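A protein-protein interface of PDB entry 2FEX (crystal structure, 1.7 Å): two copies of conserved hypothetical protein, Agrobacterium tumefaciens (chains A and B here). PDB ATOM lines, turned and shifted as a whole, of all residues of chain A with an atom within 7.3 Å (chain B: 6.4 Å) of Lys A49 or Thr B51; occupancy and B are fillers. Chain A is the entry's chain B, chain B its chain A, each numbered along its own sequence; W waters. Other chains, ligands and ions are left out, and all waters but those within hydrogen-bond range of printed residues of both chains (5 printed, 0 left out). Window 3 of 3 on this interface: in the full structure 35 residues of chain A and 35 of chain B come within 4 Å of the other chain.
CE1 of His B34 touches O of Gly A46 (3.2 Å). His B34 touches Gly A47. CD1 of Leu B8 touches CD2 of Leu A48 (3.8 Å). Leu A48 touches His B34. CD2 of Leu A48 touches CG1 of Val B50 (3.8 Å). O of Lys B49 touches O of Lys A49 (3.5 Å). O of Lys A49 touches CA of Val B50, 3.2 Å away. Val A50 touches Lys B49 (CA to O, 3.3 Å).
Lys A49 touches its own counterpart, Lys B49. Lys A49 touches Val B50, and with the chains exchanged Val A50 touches Lys B49. Lys A49 touches Thr B51, and with the chains exchanged Thr A51 touches Lys B49. Positions printed for both chains: 41, 42, 49, 50 and 51. Of the 10 pairs that touch across the chains among the printed residues, 5 have their exchanged pair printed and touching as well.
Of the printed residues of chain B, Leu A48 touches Leu B8 (3.8 Å), His B34 (3.4 Å) and Val B50 (3.8 Å). Printed residues of chain B within 4 Å of Lys A49: Lys B49 (3.5 Å), Val B50 (3.2 Å) and Thr B51 (2.9 Å). Of the printed residues of chain A, Lys B49 touches Lys A49, Val A50 and Thr A51. Of the printed residues of chain A, Val B50 touches Leu A48 and Lys A49. Of chain A, only Lys A49 comes within 4 Å of Thr B51.
The backbone carbonyl oxygen (O) of His B34 sits at hydrogen-bond distance from the backbone NH (N) of Asp B53. N of Val B50 is in hydrogen-bond range of O of Val B42 (2.9 Å). N of Val A50 is in hydrogen-bond range of O of Val A42, 2.9 Å away. The side-chain hydroxyl (OG) of Ser A44 sits close to the backbone NH (N) of Gly A46, at 3.2 Å. The backbone NH (N) of Gly A47 sits at hydrogen-bond distance from the side-chain hydroxyl (OG) of Ser A44 (3.2 Å). OG of Ser A44 lies within hydrogen-bond range of N of Leu A48 (3.0 Å).
N of Thr A51 is in hydrogen-bond range of O of Lys B49 (3.0 Å). The backbone NH (N) of Thr B51 lies within hydrogen-bond range of the backbone carbonyl oxygen (O) of Lys A49 (2.9 Å).
Printed residues of chain B that touch a printed residue of chain A: Leu B8, His B34, Lys B49, Val B50 and Thr B51. Hydrophobic or aromatic side chains of chain B within 4 Å of the printed part of chain A: Leu B8, His B34 and Val B50. Of the 12 printed residues of chain A, 6 touch a printed residue of chain B. Hydrophobic or aromatic side chains of chain A that line the printed part of chain B: Leu A48 and Val A50. Along chain A the printed residues that touch a printed residue of chain B span positions 46 to 51. Among the printed residues, no Asp or Glu carboxylate lies within 4 Å of a Lys or Arg side-chain nitrogen of the other chain.
Water W1 lies within hydrogen-bond range of the side-chain hydroxyl of Thr A51, the side-chain hydroxyl of Thr B51 and the backbone carbonyl oxygen of Lys B49. Water W3 lies within hydrogen-bond range of OD2 of Asp B53 (2.7 Å), O of Gly A47 (2.8 Å) and ND1 of His B34 (2.8 Å). Water W5 lies within hydrogen-bond range of the backbone carbonyl oxygen of Thr B51 (2.8 Å), the backbone NH of Lys A49 (2.9 Å) and the backbone carbonyl oxygen of Gly A47 (3.2 Å). Water W4 lies within hydrogen-bond range of the backbone carbonyl oxygen of Thr A51 (2.8 Å) and the backbone NH of Lys B49 (2.9 Å). Water W2 bridges OD1 of Asp B53 (2.9 Å) and O of Gly A47 (3.4 Å).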
ATOM      1  N   GLN A  10     -36.285  -9.809 -16.715  1.00  0.00           N
ATOM      2  CA  GLN A  10     -35.596 -10.689 -15.754  1.00  0.00           C
ATOM      3  C   GLN A  10     -36.644 -11.643 -15.126  1.00  0.00           C
ATOM      4  O   GLN A  10     -37.747 -11.212 -14.743  1.00  0.00           O
ATOM      5  CB  GLN A  10     -34.929  -9.791 -14.708  1.00  0.00           C
ATOM      6  CG  GLN A  10     -34.066 -10.583 -13.722  1.00  0.00           C
ATOM      7  CD  GLN A  10     -32.829 -11.247 -14.349  1.00  0.00           C
ATOM      8  OE1 GLN A  10     -32.506 -11.059 -15.532  1.00  0.00           O
ATOM      9  NE2 GLN A  10     -32.078 -11.992 -13.498  1.00  0.00           N
ATOM     10  N   PHE A  12     -38.365 -13.976 -16.519  1.00  0.00           N
ATOM     11  CA  PHE A  12     -39.579 -14.299 -17.317  1.00  0.00           C
ATOM     12  C   PHE A  12     -39.904 -15.798 -17.221  1.00  0.00           C
ATOM     13  O   PHE A  12     -39.000 -16.666 -17.007  1.00  0.00           O
ATOM     14  CB  PHE A  12     -39.517 -13.841 -18.768  1.00  0.00           C
ATOM     15  CG  PHE A  12     -38.580 -14.665 -19.664  1.00  0.00           C
ATOM     16  CD1 PHE A  12     -39.082 -15.741 -20.406  1.00  0.00           C
ATOM     17  CD2 PHE A  12     -37.254 -14.255 -19.851  1.00  0.00           C
ATOM     18  CE1 PHE A  12     -38.223 -16.485 -21.365  1.00  0.00           C
ATOM     19  CE2 PHE A  12     -36.404 -14.951 -20.751  1.00  0.00           C
ATOM     20  CZ  PHE A  12     -36.887 -16.068 -21.495  1.00  0.00           C
ATOM     21  N   PRO A  41     -29.281  -8.115 -21.846  1.00  0.00           N
ATOM     22  CA  PRO A  41     -29.701  -9.534 -21.592  1.00  0.00           C
ATOM     23  C   PRO A  41     -30.459  -9.695 -20.264  1.00  0.00           C
ATOM     24  O   PRO A  41     -30.247  -8.895 -19.307  1.00  0.00           O
ATOM     25  CB  PRO A  41     -28.331 -10.309 -21.530  1.00  0.00           C
ATOM     26  CG  PRO A  41     -27.429  -9.491 -22.346  1.00  0.00           C
ATOM     27  CD  PRO A  41     -27.830  -7.998 -22.045  1.00  0.00           C
ATOM     28  N   VAL A  42     -31.298 -10.718 -20.198  1.00  0.00           N
ATOM     29  CA  VAL A  42     -32.026 -11.063 -18.987  1.00  0.00           C
ATOM     30  C   VAL A  42     -31.881 -12.569 -18.800  1.00  0.00           C
ATOM     31  O   VAL A  42     -31.506 -13.294 -19.758  1.00  0.00           O
ATOM     32  CB  VAL A  42     -33.523 -10.703 -19.081  1.00  0.00           C
ATOM     33  CG1 VAL A  42     -33.668  -9.189 -19.159  1.00  0.00           C
ATOM     34  CG2 VAL A  42     -34.174 -11.404 -20.311  1.00  0.00           C
ATOM     35  N   THR A  43     -32.221 -13.036 -17.600  1.00  0.00           N
ATOM     36  CA  THR A  43     -32.117 -14.468 -17.300  1.00  0.00           C
ATOM     37  C   THR A  43     -33.503 -14.952 -16.948  1.00  0.00           C
ATOM     38  O   THR A  43     -34.151 -14.368 -16.073  1.00  0.00           O
ATOM     39  CB  THR A  43     -31.145 -14.728 -16.184  1.00  0.00           C
ATOM     40  OG1 THR A  43     -29.812 -14.316 -16.621  1.00  0.00           O
ATOM     41  CG2 THR A  43     -31.095 -16.231 -15.905  1.00  0.00           C
ATOM     42  N   SER A  44     -33.989 -15.942 -17.659  1.00  0.00           N
ATOM     43  CA  SER A  44     -35.352 -16.430 -17.382  1.00  0.00           C
ATOM     44  C   SER A  44     -35.468 -17.106 -15.987  1.00  0.00           C
ATOM     45  O   SER A  44     -34.443 -17.449 -15.360  1.00  0.00           O
ATOM     46  CB  SER A  44     -35.731 -17.479 -18.434  1.00  0.00           C
ATOM     47  OG  SER A  44     -35.033 -18.711 -18.208  1.00  0.00           O
ATOM     48  N   GLY A  46     -36.062 -20.145 -15.579  1.00  0.00           N
ATOM     49  CA  GLY A  46     -35.305 -21.393 -15.764  1.00  0.00           C
ATOM     50  C   GLY A  46     -33.810 -21.256 -15.983  1.00  0.00           C
ATOM     51  O   GLY A  46     -33.106 -22.302 -16.074  1.00  0.00           O
ATOM     52  N   GLY A  47     -33.293 -20.022 -15.870  1.00  0.00           N
ATOM     53  CA  GLY A  47     -31.834 -19.738 -15.986  1.00  0.00           C
ATOM     54  C   GLY A  47     -31.288 -19.499 -17.414  1.00  0.00           C
ATOM     55  O   GLY A  47     -30.044 -19.389 -17.597  1.00  0.00           O
ATOM     56  N   LEU A  48     -32.153 -19.391 -18.420  1.00  0.00           N
ATOM     57  CA  LEU A  48     -31.667 -19.120 -19.767  1.00  0.00           C
ATOM     58  C   LEU A  48     -31.205 -17.676 -19.798  1.00  0.00           C
ATOM     59  O   LEU A  48     -31.989 -16.757 -19.476  1.00  0.00           O
ATOM     60  CB  LEU A  48     -32.801 -19.229 -20.798  1.00  0.00           C
ATOM     61  CG  LEU A  48     -33.347 -20.584 -21.145  1.00  0.00           C
ATOM     62  CD1 LEU A  48     -34.545 -20.348 -22.188  1.00  0.00           C
ATOM     63  CD2 LEU A  48     -32.290 -21.518 -21.798  1.00  0.00           C
ATOM     64  N   LYS A  49     -29.984 -17.469 -20.271  1.00  0.00           N
ATOM     65  CA  LYS A  49     -29.474 -16.088 -20.457  1.00  0.00           C
ATOM     66  C   LYS A  49     -29.788 -15.710 -21.927  1.00  0.00           C
ATOM     67  O   LYS A  49     -29.214 -16.306 -22.855  1.00  0.00           O
ATOM     68  CB  LYS A  49     -27.974 -16.052 -20.188  1.00  0.00           C
ATOM     69  CG  LYS A  49     -27.382 -14.673 -20.676  1.00  0.00           C
ATOM     70  CD  LYS A  49     -26.199 -14.374 -19.890  1.00  0.00           C
ATOM     71  CE  LYS A  49     -26.680 -13.623 -18.676  1.00  0.00           C
ATOM     72  NZ  LYS A  49     -25.507 -12.902 -18.226  1.00  0.00           N
ATOM     73  N   VAL A  50     -30.682 -14.720 -22.109  1.00  0.00           N
ATOM     74  CA  VAL A  50     -31.172 -14.392 -23.411  1.00  0.00           C
ATOM     75  C   VAL A  50     -30.763 -12.949 -23.779  1.00  0.00           C
ATOM     76  O   VAL A  50     -30.921 -12.002 -22.969  1.00  0.00           O
ATOM     77  CB  VAL A  50     -32.717 -14.425 -23.397  1.00  0.00           C
ATOM     78  CG1 VAL A  50     -33.245 -13.998 -24.756  1.00  0.00           C
ATOM     79  CG2 VAL A  50     -33.226 -15.882 -23.073  1.00  0.00           C
ATOM     80  N   THR A  51     -30.228 -12.788 -24.978  1.00  0.00           N
ATOM     81  CA  THR A  51     -29.894 -11.444 -25.453  1.00  0.00           C
ATOM     82  C   THR A  51     -30.997 -11.014 -26.388  1.00  0.00           C
ATOM     83  O   THR A  51     -31.225 -11.688 -27.387  1.00  0.00           O
ATOM     84  CB  THR A  51     -28.561 -11.496 -26.227  1.00  0.00           C
ATOM     85  OG1 THR A  51     -27.559 -11.931 -25.293  1.00  0.00           O
ATOM     86  CG2 THR A  51     -28.199 -10.078 -26.683  1.00  0.00           C
ATOM     87  N   LEU B   8     -28.899 -27.902 -24.603  1.00  0.00           N
ATOM     88  CA  LEU B   8     -29.486 -27.133 -25.715  1.00  0.00           C
ATOM     89  C   LEU B   8     -28.730 -27.370 -27.005  1.00  0.00           C
ATOM     90  O   LEU B   8     -27.625 -27.973 -27.036  1.00  0.00           O
ATOM     91  CB  LEU B   8     -29.394 -25.611 -25.376  1.00  0.00           C
ATOM     92  CG  LEU B   8     -30.110 -25.181 -24.067  1.00  0.00           C
ATOM     93  CD1 LEU B   8     -29.878 -23.653 -23.802  1.00  0.00           C
ATOM     94  CD2 LEU B   8     -31.669 -25.571 -24.043  1.00  0.00           C
ATOM     95  N   HIS B  34     -27.069 -24.893 -18.257  1.00  0.00           N
ATOM     96  CA  HIS B  34     -27.406 -25.003 -19.663  1.00  0.00           C
ATOM     97  C   HIS B  34     -26.097 -25.170 -20.443  1.00  0.00           C
ATOM     98  O   HIS B  34     -25.119 -24.449 -20.191  1.00  0.00           O
ATOM     99  CB  HIS B  34     -28.148 -23.741 -20.174  1.00  0.00           C
ATOM    100  CG  HIS B  34     -29.594 -23.747 -19.783  1.00  0.00           C
ATOM    101  ND1 HIS B  34     -30.051 -23.010 -18.713  1.00  0.00           N
ATOM    102  CD2 HIS B  34     -30.665 -24.390 -20.305  1.00  0.00           C
ATOM    103  CE1 HIS B  34     -31.352 -23.222 -18.575  1.00  0.00           C
ATOM    104  NE2 HIS B  34     -31.757 -24.053 -19.526  1.00  0.00           N
ATOM    105  N   THR B  36     -24.342 -26.093 -24.583  1.00  0.00           N
ATOM    106  CA  THR B  36     -24.507 -26.278 -26.032  1.00  0.00           C
ATOM    107  C   THR B  36     -23.285 -27.123 -26.467  1.00  0.00           C
ATOM    108  O   THR B  36     -22.268 -27.221 -25.748  1.00  0.00           O
ATOM    109  CB  THR B  36     -24.512 -24.921 -26.785  1.00  0.00           C
ATOM    110  OG1 THR B  36     -23.227 -24.246 -26.513  1.00  0.00           O
ATOM    111  CG2 THR B  36     -25.703 -24.025 -26.334  1.00  0.00           C
ATOM    112  N   GLY B  39     -20.325 -24.837 -26.483  1.00  0.00           N
ATOM    113  CA  GLY B  39     -20.262 -23.890 -25.381  1.00  0.00           C
ATOM    114  C   GLY B  39     -20.609 -22.461 -25.773  1.00  0.00           C
ATOM    115  O   GLY B  39     -20.589 -21.564 -24.920  1.00  0.00           O
ATOM    116  N   MET B  40     -20.906 -22.238 -27.047  1.00  0.00           N
ATOM    117  CA  MET B  40     -21.264 -20.887 -27.485  1.00  0.00           C
ATOM    118  C   MET B  40     -22.777 -20.765 -27.712  1.00  0.00           C
ATOM    119  O   MET B  40     -23.511 -21.791 -27.632  1.00  0.00           O
ATOM    120  CB  MET B  40     -20.402 -20.486 -28.718  1.00  0.00           C
ATOM    121  CG  MET B  40     -18.920 -20.247 -28.281  1.00  0.00           C
ATOM    122  SD  MET B  40     -17.751 -19.781 -29.681  1.00  0.00           S
ATOM    123  CE  MET B  40     -17.248 -21.658 -30.269  1.00  0.00           C
ATOM    124  N   PRO B  41     -23.261 -19.542 -27.946  1.00  0.00           N
ATOM    125  CA  PRO B  41     -24.720 -19.314 -27.997  1.00  0.00           C
ATOM    126  C   PRO B  41     -25.401 -20.154 -29.086  1.00  0.00           C
ATOM    127  O   PRO B  41     -24.782 -20.540 -30.119  1.00  0.00           O
ATOM    128  CB  PRO B  41     -24.832 -17.794 -28.330  1.00  0.00           C
ATOM    129  CG  PRO B  41     -23.591 -17.247 -27.597  1.00  0.00           C
ATOM    130  CD  PRO B  41     -22.531 -18.268 -28.073  1.00  0.00           C
ATOM    131  N   VAL B  42     -26.691 -20.380 -28.844  1.00  0.00           N
ATOM    132  CA  VAL B  42     -27.552 -20.959 -29.869  1.00  0.00           C
ATOM    133  C   VAL B  42     -28.885 -20.210 -29.919  1.00  0.00           C
ATOM    134  O   VAL B  42     -29.244 -19.510 -28.976  1.00  0.00           O
ATOM    135  CB  VAL B  42     -27.855 -22.450 -29.560  1.00  0.00           C
ATOM    136  CG1 VAL B  42     -26.526 -23.281 -29.700  1.00  0.00           C
ATOM    137  CG2 VAL B  42     -28.538 -22.647 -28.198  1.00  0.00           C
ATOM    138  N   LYS B  49     -31.951 -15.886 -28.365  1.00  0.00           N
ATOM    139  CA  LYS B  49     -30.469 -16.033 -28.478  1.00  0.00           C
ATOM    140  C   LYS B  49     -29.909 -16.349 -27.085  1.00  0.00           C
ATOM    141  O   LYS B  49     -29.839 -15.484 -26.217  1.00  0.00           O
ATOM    142  CB  LYS B  49     -29.856 -14.728 -29.048  1.00  0.00           C
ATOM    143  CG  LYS B  49     -30.442 -14.257 -30.399  1.00  0.00           C
ATOM    144  CD  LYS B  49     -30.687 -15.369 -31.359  1.00  0.00           C
ATOM    145  CE  LYS B  49     -31.109 -14.797 -32.741  1.00  0.00           C
ATOM    146  NZ  LYS B  49     -32.538 -14.284 -32.726  1.00  0.00           N
ATOM    147  N   VAL B  50     -29.612 -17.629 -26.851  1.00  0.00           N
ATOM    148  CA  VAL B  50     -29.238 -18.092 -25.523  1.00  0.00           C
ATOM    149  C   VAL B  50     -27.731 -18.301 -25.386  1.00  0.00           C
ATOM    150  O   VAL B  50     -27.117 -19.023 -26.218  1.00  0.00           O
ATOM    151  CB  VAL B  50     -29.942 -19.426 -25.236  1.00  0.00           C
ATOM    152  CG1 VAL B  50     -29.548 -19.900 -23.829  1.00  0.00           C
ATOM    153  CG2 VAL B  50     -31.510 -19.217 -25.398  1.00  0.00           C
ATOM    154  N   THR B  51     -27.142 -17.679 -24.363  1.00  0.00           N
ATOM    155  CA  THR B  51     -25.720 -17.940 -24.057  1.00  0.00           C
ATOM    156  C   THR B  51     -25.765 -19.011 -22.953  1.00  0.00           C
ATOM    157  O   THR B  51     -26.267 -18.761 -21.836  1.00  0.00           O
ATOM    158  CB  THR B  51     -25.075 -16.647 -23.528  1.00  0.00           C
ATOM    159  OG1 THR B  51     -24.995 -15.716 -24.604  1.00  0.00           O
ATOM    160  CG2 THR B  51     -23.661 -16.978 -23.008  1.00  0.00           C
ATOM    161  N   PRO B  52     -25.206 -20.204 -23.221  1.00  0.00           N
ATOM    162  CA  PRO B  52     -25.225 -21.250 -22.206  1.00  0.00           C
ATOM    163  C   PRO B  52     -24.146 -21.016 -21.113  1.00  0.00           C
ATOM    164  O   PRO B  52     -23.271 -20.115 -21.235  1.00  0.00           O
ATOM    165  CB  PRO B  52     -24.851 -22.502 -23.000  1.00  0.00           C
ATOM    166  CG  PRO B  52     -23.809 -21.978 -23.976  1.00  0.00           C
ATOM    167  CD  PRO B  52     -24.448 -20.626 -24.429  1.00  0.00           C
ATOM    168  N   ASP B  53     -24.186 -21.846 -20.077  1.00  0.00           N
ATOM    169  CA  ASP B  53     -23.146 -21.860 -19.077  1.00  0.00           C
ATOM    170  C   ASP B  53     -21.862 -22.553 -19.519  1.00  0.00           C
ATOM    171  O   ASP B  53     -20.770 -22.143 -19.125  1.00  0.00           O
ATOM    172  CB  ASP B  53     -23.665 -22.592 -17.831  1.00  0.00           C
ATOM    173  CG  ASP B  53     -24.903 -21.908 -17.252  1.00  0.00           C
ATOM    174  OD1 ASP B  53     -24.736 -20.725 -16.810  1.00  0.00           O
ATOM    175  OD2 ASP B  53     -25.985 -22.500 -17.275  1.00  0.00           O
HETATM  176  O   HOH W   1     -27.258 -14.574 -25.583  1.00  0.00           O
HETATM  177  O   HOH W   2     -26.737 -18.969 -17.991  1.00  0.00           O
HETATM  178  O   HOH W   3     -28.502 -21.585 -16.906  1.00  0.00           O
HETATM  179  O   HOH W   4     -33.364 -13.304 -28.259  1.00  0.00           O
HETATM  180  O   HOH W   5     -28.317 -19.837 -20.288  1.00  0.00           O
